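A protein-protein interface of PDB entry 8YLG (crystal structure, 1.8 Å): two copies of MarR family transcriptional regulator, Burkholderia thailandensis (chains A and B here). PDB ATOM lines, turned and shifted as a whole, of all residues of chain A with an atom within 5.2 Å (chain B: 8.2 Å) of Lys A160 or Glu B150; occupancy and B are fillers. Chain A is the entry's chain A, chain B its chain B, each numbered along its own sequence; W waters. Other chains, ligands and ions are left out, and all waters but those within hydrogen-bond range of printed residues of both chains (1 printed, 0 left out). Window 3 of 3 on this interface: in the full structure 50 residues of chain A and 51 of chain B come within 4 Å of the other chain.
Water W1 bridges the side-chain carboxylate (OD1) of Asp A159 (2.4 Å) and the side-chain carboxylate (OD2) of Asp B7 (2.8 Å).
The backbone carbonyl oxygen of Ala A155 is in hydrogen-bond range of the guanidinium group of Arg B33 (3.0 Å).
The side-chain amino group (NZ) of Lys A160 lies within salt-bridge range of the side-chain carboxylate (OE2) of Glu B150, 2.8 Å away.
Leu B146 touches Leu A157.
Leu A157 touches Glu B150.
Leu A157 touches Gln B153 (CD1 to NE2, 3.9 Å).
N of Leu B154 touches CD1 of Leu A157 (3.8 Å).
Asp A159 touches Arg B33 (CB to NH1, 3.6 Å).
Ala B145 touches Lys A160.
CD2 of Leu B146 touches CG of Lys A160, at 3.8 Å.
Val B142 touches Leu A161.
CD1 of Leu A162 touches O of Arg B33, at 3.9 Å.
CA of Gly A164 touches CB of Ala B145, 3.8 Å away.
N of Ser B147 is in hydrogen-bond range of OE1 of Glu B150.
The side-chain carboxylate (OD2) of Asp A159 lies within hydrogen-bond range of the side-chain amide nitrogen (NE2) of Gln A163.
The guanidinium group (NE) of Arg B33 is in salt-bridge range of the side-chain carboxylate (OD2) of Asp B7 (2.8 Å).
O of Leu B146 sits at hydrogen-bond distance from NE2 of Gln B151 (3.0 Å).
Leu B157 touches its own counterpart, Leu A157.
Positions printed for both chains: 155, 156 and 157.
Printed residues of chain B that touch a printed residue of chain A: Arg B33, Val B142, Ala B145, Leu B146, Glu B150, Gln B153, Leu B154 and Leu B157.
Hydrophobic or aromatic side chains of chain B within 4 Å of the printed part of chain A: Ala B145, Leu B146 and Leu B157.
Of the 10 printed residues of chain A, 8 touch a printed residue of chain B.
Printed residues of chain A that touch a printed residue of chain B: Ala A155, Leu A157, Leu A158, Asp A159, Lys A160, Leu A161, Leu A162 and Gly A164.
Among the printed residues, 14 pairs touch across the chains.
Of chain B, only Ala B145, Leu B146 and Glu B150 come within 4 Å of Lys A160.
Glu B150 touches just these residues of chain A: Leu A157 (3.7 Å) and Lys A160 (2.8 Å).
Printed residues of chain B within 4 Å of Leu A161: Val B142.
Printed residues of chain B within 4 Å of Ala A155: Arg B33 (3.0 Å).
Of the printed residues of chain B, Asp A159 touches Arg B33 (3.6 Å).
Of the printed residues of chain A, Arg B33 touches Ala A155, Leu A158, Asp A159 and Leu A162.
Ala B148 touches none of the printed residues of chain A.
The nearest residue of chain B that does not touch Lys A160 is Ser B147 (5.3 Å).
The nearest printed residue of chain A that does not touch Glu B150 is Lys A156 (7.3 Å).
The nearest printed residue of chain A that does not touch Leu B146 is Leu A161 (4.3 Å).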
ATOM      1  N   ALA A 155      19.490   0.389  18.361  1.00  0.00           N
ATOM      2  CA  ALA A 155      19.736   1.569  19.184  1.00  0.00           C
ATOM      3  C   ALA A 155      18.430   2.179  19.674  1.00  0.00           C
ATOM      4  O   ALA A 155      18.334   2.609  20.831  1.00  0.00           O
ATOM      5  CB  ALA A 155      20.542   2.603  18.395  1.00  0.00           C
ATOM      6  N   LYS A 156      17.415   2.232  18.802  1.00  0.00           N
ATOM      7  CA  LYS A 156      16.129   2.808  19.181  1.00  0.00           C
ATOM      8  C   LYS A 156      15.432   1.953  20.226  1.00  0.00           C
ATOM      9  O   LYS A 156      14.878   2.479  21.200  1.00  0.00           O
ATOM     10  CB  LYS A 156      15.235   2.971  17.949  1.00  0.00           C
ATOM     11  N   LEU A 157      15.431   0.630  20.030  1.00  0.00           N
ATOM     12  CA  LEU A 157      14.771  -0.258  20.982  1.00  0.00           C
ATOM     13  C   LEU A 157      15.438  -0.182  22.352  1.00  0.00           C
ATOM     14  O   LEU A 157      14.754  -0.181  23.383  1.00  0.00           O
ATOM     15  CB  LEU A 157      14.780  -1.686  20.444  1.00  0.00           C
ATOM     16  CG  LEU A 157      13.888  -1.972  19.232  1.00  0.00           C
ATOM     17  CD1 LEU A 157      14.243  -3.324  18.637  1.00  0.00           C
ATOM     18  CD2 LEU A 157      12.413  -1.958  19.622  1.00  0.00           C
ATOM     19  N   LEU A 158      16.777  -0.103  22.381  1.00  0.00           N
ATOM     20  CA  LEU A 158      17.489   0.004  23.654  1.00  0.00           C
ATOM     21  C   LEU A 158      17.212   1.338  24.334  1.00  0.00           C
ATOM     22  O   LEU A 158      17.090   1.402  25.563  1.00  0.00           O
ATOM     23  CB  LEU A 158      18.986  -0.191  23.441  1.00  0.00           C
ATOM     24  CG  LEU A 158      19.358  -1.631  23.093  1.00  0.00           C
ATOM     25  CD1 LEU A 158      20.802  -1.732  22.614  1.00  0.00           C
ATOM     26  CD2 LEU A 158      19.101  -2.545  24.283  1.00  0.00           C
ATOM     27  N   ASP A 159      17.096   2.412  23.552  1.00  0.00           N
ATOM     28  CA  ASP A 159      16.756   3.708  24.127  1.00  0.00           C
ATOM     29  C   ASP A 159      15.363   3.679  24.742  1.00  0.00           C
ATOM     30  O   ASP A 159      15.160   4.160  25.864  1.00  0.00           O
ATOM     31  CB  ASP A 159      16.869   4.783  23.044  1.00  0.00           C
ATOM     32  CG  ASP A 159      16.308   6.131  23.478  1.00  0.00           C
ATOM     33  OD1 ASP A 159      16.690   6.639  24.547  1.00  0.00           O
ATOM     34  OD2 ASP A 159      15.478   6.684  22.737  1.00  0.00           O
ATOM     35  N   LYS A 160      14.395   3.088  24.037  1.00  0.00           N
ATOM     36  CA  LYS A 160      13.042   2.987  24.585  1.00  0.00           C
ATOM     37  C   LYS A 160      13.043   2.193  25.887  1.00  0.00           C
ATOM     38  O   LYS A 160      12.336   2.541  26.844  1.00  0.00           O
ATOM     39  CB  LYS A 160      12.107   2.350  23.548  1.00  0.00           C
ATOM     40  CG  LYS A 160      10.615   2.519  23.809  1.00  0.00           C
ATOM     41  CD  LYS A 160       9.768   2.126  22.579  1.00  0.00           C
ATOM     42  CE  LYS A 160       8.289   2.434  22.806  1.00  0.00           C
ATOM     43  NZ  LYS A 160       7.364   2.012  21.698  1.00  0.00           N
ATOM     44  N   LEU A 161      13.830   1.121  25.937  1.00  0.00           N
ATOM     45  CA  LEU A 161      13.925   0.312  27.146  1.00  0.00           C
ATOM     46  C   LEU A 161      14.587   1.092  28.276  1.00  0.00           C
ATOM     47  O   LEU A 161      14.158   1.003  29.432  1.00  0.00           O
ATOM     48  CB  LEU A 161      14.698  -0.973  26.838  1.00  0.00           C
ATOM     49  CG  LEU A 161      14.874  -2.027  27.923  1.00  0.00           C
ATOM     50  CD1 LEU A 161      13.543  -2.610  28.313  1.00  0.00           C
ATOM     51  CD2 LEU A 161      15.825  -3.129  27.442  1.00  0.00           C
ATOM     52  N   LEU A 162      15.627   1.870  27.961  1.00  0.00           N
ATOM     53  CA  LEU A 162      16.282   2.679  28.986  1.00  0.00           C
ATOM     54  C   LEU A 162      15.363   3.789  29.493  1.00  0.00           C
ATOM     55  O   LEU A 162      15.309   4.051  30.700  1.00  0.00           O
ATOM     56  CB  LEU A 162      17.580   3.263  28.436  1.00  0.00           C
ATOM     57  CG  LEU A 162      18.759   2.288  28.399  1.00  0.00           C
ATOM     58  CD1 LEU A 162      19.907   2.893  27.594  1.00  0.00           C
ATOM     59  CD2 LEU A 162      19.214   1.896  29.789  1.00  0.00           C
ATOM     60  N   GLN A 163      14.637   4.455  28.588  1.00  0.00           N
ATOM     61  CA  GLN A 163      13.686   5.476  29.018  1.00  0.00           C
ATOM     62  C   GLN A 163      12.621   4.864  29.908  1.00  0.00           C
ATOM     63  O   GLN A 163      12.150   5.506  30.853  1.00  0.00           O
ATOM     64  CB  GLN A 163      13.037   6.152  27.808  1.00  0.00           C
ATOM     65  CG  GLN A 163      13.972   7.004  26.959  1.00  0.00           C
ATOM     66  CD  GLN A 163      13.221   7.799  25.899  1.00  0.00           C
ATOM     67  OE1 GLN A 163      12.149   8.352  26.163  1.00  0.00           O
ATOM     68  NE2 GLN A 163      13.774   7.849  24.692  1.00  0.00           N
ATOM     69  N   GLY A 164      12.221   3.624  29.609  1.00  0.00           N
ATOM     70  CA  GLY A 164      11.319   2.906  30.497  1.00  0.00           C
ATOM     71  C   GLY A 164      11.844   2.795  31.916  1.00  0.00           C
ATOM     72  O   GLY A 164      11.106   3.014  32.877  1.00  0.00           O
ATOM     73  N   ASP B   7      20.406  10.971  25.707  1.00  0.00           N
ATOM     74  CA  ASP B   7      20.813  10.108  26.803  1.00  0.00           C
ATOM     75  C   ASP B   7      22.340  10.102  26.919  1.00  0.00           C
ATOM     76  O   ASP B   7      23.045  10.844  26.224  1.00  0.00           O
ATOM     77  CB  ASP B   7      20.225   8.700  26.627  1.00  0.00           C
ATOM     78  CG  ASP B   7      20.842   7.923  25.465  1.00  0.00           C
ATOM     79  OD1 ASP B   7      21.499   8.531  24.587  1.00  0.00           O
ATOM     80  OD2 ASP B   7      20.663   6.682  25.435  1.00  0.00           O
ATOM     81  N   ARG B  33      24.450   1.885  24.745  1.00  0.00           N
ATOM     82  CA  ARG B  33      23.112   1.633  25.277  1.00  0.00           C
ATOM     83  C   ARG B  33      22.953   0.180  25.686  1.00  0.00           C
ATOM     84  O   ARG B  33      22.295  -0.111  26.688  1.00  0.00           O
ATOM     85  CB  ARG B  33      22.036   2.016  24.263  1.00  0.00           C
ATOM     86  CG  ARG B  33      21.870   3.524  24.104  1.00  0.00           C
ATOM     87  CD  ARG B  33      20.758   3.885  23.139  1.00  0.00           C
ATOM     88  NE  ARG B  33      20.674   5.340  23.009  1.00  0.00           N
ATOM     89  CZ  ARG B  33      20.205   5.975  21.943  1.00  0.00           C
ATOM     90  NH1 ARG B  33      19.748   5.293  20.905  1.00  0.00           N
ATOM     91  NH2 ARG B  33      20.210   7.302  21.914  1.00  0.00           N
ATOM     92  N   VAL B 142       9.884  -4.884  33.582  1.00  0.00           N
ATOM     93  CA  VAL B 142      11.060  -4.274  32.960  1.00  0.00           C
ATOM     94  C   VAL B 142      10.837  -4.081  31.466  1.00  0.00           C
ATOM     95  O   VAL B 142      11.136  -3.021  30.909  1.00  0.00           O
ATOM     96  CB  VAL B 142      12.309  -5.143  33.226  1.00  0.00           C
ATOM     97  CG1 VAL B 142      13.454  -4.770  32.276  1.00  0.00           C
ATOM     98  CG2 VAL B 142      12.738  -5.004  34.671  1.00  0.00           C
ATOM     99  N   LEU B 143      10.260  -5.085  30.806  1.00  0.00           N
ATOM    100  CA  LEU B 143      10.078  -5.067  29.365  1.00  0.00           C
ATOM    101  C   LEU B 143       8.803  -4.358  28.928  1.00  0.00           C
ATOM    102  O   LEU B 143       8.616  -4.148  27.724  1.00  0.00           O
ATOM    103  CB  LEU B 143      10.055  -6.497  28.833  1.00  0.00           C
ATOM    104  CG  LEU B 143      11.372  -7.237  29.001  1.00  0.00           C
ATOM    105  CD1 LEU B 143      11.147  -8.710  28.720  1.00  0.00           C
ATOM    106  CD2 LEU B 143      12.403  -6.652  28.043  1.00  0.00           C
ATOM    107  N   SER B 144       7.939  -3.978  29.877  1.00  0.00           N
ATOM    108  CA  SER B 144       6.623  -3.435  29.548  1.00  0.00           C
ATOM    109  C   SER B 144       6.702  -2.120  28.779  1.00  0.00           C
ATOM    110  O   SER B 144       5.708  -1.713  28.177  1.00  0.00           O
ATOM    111  CB  SER B 144       5.794  -3.268  30.829  1.00  0.00           C
ATOM    112  OG  SER B 144       6.337  -2.254  31.661  1.00  0.00           O
ATOM    113  N   ALA B 145       7.856  -1.447  28.774  1.00  0.00           N
ATOM    114  CA  ALA B 145       7.989  -0.252  27.950  1.00  0.00           C
ATOM    115  C   ALA B 145       7.992  -0.580  26.464  1.00  0.00           C
ATOM    116  O   ALA B 145       7.777   0.317  25.640  1.00  0.00           O
ATOM    117  CB  ALA B 145       9.277   0.492  28.304  1.00  0.00           C
ATOM    118  N   LEU B 146       8.239  -1.835  26.106  1.00  0.00           N
ATOM    119  CA  LEU B 146       8.219  -2.286  24.720  1.00  0.00           C
ATOM    120  C   LEU B 146       6.947  -3.077  24.444  1.00  0.00           C
ATOM    121  O   LEU B 146       6.497  -3.851  25.291  1.00  0.00           O
ATOM    122  CB  LEU B 146       9.432  -3.163  24.430  1.00  0.00           C
ATOM    123  CG  LEU B 146      10.822  -2.547  24.600  1.00  0.00           C
ATOM    124  CD1 LEU B 146      11.886  -3.540  24.155  1.00  0.00           C
ATOM    125  CD2 LEU B 146      10.943  -1.247  23.833  1.00  0.00           C
ATOM    126  N   SER B 147       6.396  -2.914  23.241  1.00  0.00           N
ATOM    127  CA  SER B 147       5.261  -3.732  22.836  1.00  0.00           C
ATOM    128  C   SER B 147       5.718  -5.171  22.621  1.00  0.00           C
ATOM    129  O   SER B 147       6.912  -5.460  22.554  1.00  0.00           O
ATOM    130  CB  SER B 147       4.640  -3.201  21.547  1.00  0.00           C
ATOM    131  OG  SER B 147       5.541  -3.399  20.470  1.00  0.00           O
ATOM    132  N   ALA B 148       4.745  -6.085  22.498  1.00  0.00           N
ATOM    133  CA  ALA B 148       5.092  -7.475  22.219  1.00  0.00           C
ATOM    134  C   ALA B 148       5.943  -7.584  20.957  1.00  0.00           C
ATOM    135  O   ALA B 148       6.953  -8.296  20.940  1.00  0.00           O
ATOM    136  CB  ALA B 148       3.825  -8.323  22.088  1.00  0.00           C
ATOM    137  N   ALA B 149       5.555  -6.877  19.892  1.00  0.00           N
ATOM    138  CA  ALA B 149       6.316  -6.935  18.647  1.00  0.00           C
ATOM    139  C   ALA B 149       7.721  -6.360  18.817  1.00  0.00           C
ATOM    140  O   ALA B 149       8.679  -6.878  18.237  1.00  0.00           O
ATOM    141  CB  ALA B 149       5.559  -6.207  17.536  1.00  0.00           C
ATOM    142  N   GLU B 150       7.861  -5.277  19.587  1.00  0.00           N
ATOM    143  CA  GLU B 150       9.187  -4.703  19.818  1.00  0.00           C
ATOM    144  C   GLU B 150      10.072  -5.648  20.626  1.00  0.00           C
ATOM    145  O   GLU B 150      11.281  -5.744  20.376  1.00  0.00           O
ATOM    146  CB  GLU B 150       9.056  -3.354  20.525  1.00  0.00           C
ATOM    147  CG  GLU B 150       8.498  -2.253  19.629  1.00  0.00           C
ATOM    148  CD  GLU B 150       8.135  -0.989  20.399  1.00  0.00           C
ATOM    149  OE1 GLU B 150       7.827  -1.078  21.608  1.00  0.00           O
ATOM    150  OE2 GLU B 150       8.143   0.094  19.791  1.00  0.00           O
ATOM    151  N   GLN B 151       9.501  -6.329  21.618  1.00  0.00           N
ATOM    152  CA  GLN B 151      10.283  -7.302  22.373  1.00  0.00           C
ATOM    153  C   GLN B 151      10.746  -8.443  21.476  1.00  0.00           C
ATOM    154  O   GLN B 151      11.887  -8.913  21.597  1.00  0.00           O
ATOM    155  CB  GLN B 151       9.474  -7.846  23.548  1.00  0.00           C
ATOM    156  CG  GLN B 151       9.024  -6.797  24.549  1.00  0.00           C
ATOM    157  CD  GLN B 151       8.221  -7.401  25.684  1.00  0.00           C
ATOM    158  OE1 GLN B 151       8.465  -8.536  26.095  1.00  0.00           O
ATOM    159  NE2 GLN B 151       7.240  -6.652  26.184  1.00  0.00           N
ATOM    160  N   ARG B 152       9.869  -8.914  20.581  1.00  0.00           N
ATOM    161  CA  ARG B 152      10.279  -9.951  19.635  1.00  0.00           C
ATOM    162  C   ARG B 152      11.376  -9.435  18.712  1.00  0.00           C
ATOM    163  O   ARG B 152      12.356 -10.138  18.443  1.00  0.00           O
ATOM    164  CB  ARG B 152       9.083 -10.454  18.820  1.00  0.00           C
ATOM    165  CG  ARG B 152       8.080 -11.275  19.622  1.00  0.00           C
ATOM    166  CD  ARG B 152       7.069 -11.990  18.711  1.00  0.00           C
ATOM    167  NE  ARG B 152       6.152 -11.063  18.047  1.00  0.00           N
ATOM    168  CZ  ARG B 152       4.998 -10.649  18.569  1.00  0.00           C
ATOM    169  NH1 ARG B 152       4.614 -11.080  19.765  1.00  0.00           N
ATOM    170  NH2 ARG B 152       4.225  -9.805  17.895  1.00  0.00           N
ATOM    171  N   GLN B 153      11.232  -8.202  18.225  1.00  0.00           N
ATOM    172  CA  GLN B 153      12.260  -7.630  17.364  1.00  0.00           C
ATOM    173  C   GLN B 153      13.575  -7.456  18.116  1.00  0.00           C
ATOM    174  O   GLN B 153      14.650  -7.748  17.575  1.00  0.00           O
ATOM    175  CB  GLN B 153      11.778  -6.296  16.798  1.00  0.00           C
ATOM    176  CG  GLN B 153      12.743  -5.680  15.805  1.00  0.00           C
ATOM    177  CD  GLN B 153      12.265  -4.335  15.280  1.00  0.00           C
ATOM    178  OE1 GLN B 153      12.718  -3.871  14.230  1.00  0.00           O
ATOM    179  NE2 GLN B 153      11.344  -3.704  16.010  1.00  0.00           N
ATOM    180  N   LEU B 154      13.513  -6.991  19.367  1.00  0.00           N
ATOM    181  CA  LEU B 154      14.731  -6.861  20.159  1.00  0.00           C
ATOM    182  C   LEU B 154      15.406  -8.213  20.354  1.00  0.00           C
ATOM    183  O   LEU B 154      16.636  -8.325  20.242  1.00  0.00           O
ATOM    184  CB  LEU B 154      14.416  -6.222  21.510  1.00  0.00           C
ATOM    185  CG  LEU B 154      15.588  -6.038  22.473  1.00  0.00           C
ATOM    186  CD1 LEU B 154      16.740  -5.303  21.795  1.00  0.00           C
ATOM    187  CD2 LEU B 154      15.143  -5.264  23.713  1.00  0.00           C
ATOM    188  N   ALA B 155      14.614  -9.249  20.636  1.00  0.00           N
ATOM    189  CA  ALA B 155      15.154 -10.595  20.789  1.00  0.00           C
ATOM    190  C   ALA B 155      15.828 -11.073  19.508  1.00  0.00           C
ATOM    191  O   ALA B 155      16.883 -11.710  19.561  1.00  0.00           O
ATOM    192  CB  ALA B 155      14.041 -11.564  21.200  1.00  0.00           C
ATOM    193  N   LYS B 156      15.221 -10.796  18.348  1.00  0.00           N
ATOM    194  CA  LYS B 156      15.814 -11.228  17.087  1.00  0.00           C
ATOM    195  C   LYS B 156      17.113 -10.488  16.815  1.00  0.00           C
ATOM    196  O   LYS B 156      18.111 -11.104  16.415  1.00  0.00           O
ATOM    197  CB  LYS B 156      14.826 -11.022  15.936  1.00  0.00           C
ATOM    198  N   LEU B 157      17.119  -9.166  17.025  1.00  0.00           N
ATOM    199  CA  LEU B 157      18.328  -8.383  16.776  1.00  0.00           C
ATOM    200  C   LEU B 157      19.456  -8.797  17.707  1.00  0.00           C
ATOM    201  O   LEU B 157      20.623  -8.844  17.298  1.00  0.00           O
ATOM    202  CB  LEU B 157      18.037  -6.893  16.924  1.00  0.00           C
ATOM    203  CG  LEU B 157      17.172  -6.261  15.830  1.00  0.00           C
ATOM    204  CD1 LEU B 157      16.759  -4.852  16.270  1.00  0.00           C
ATOM    205  CD2 LEU B 157      17.884  -6.226  14.488  1.00  0.00           C
HETATM  206  O   HOH W   1      18.140   6.050  26.419  1.00  0.00           O
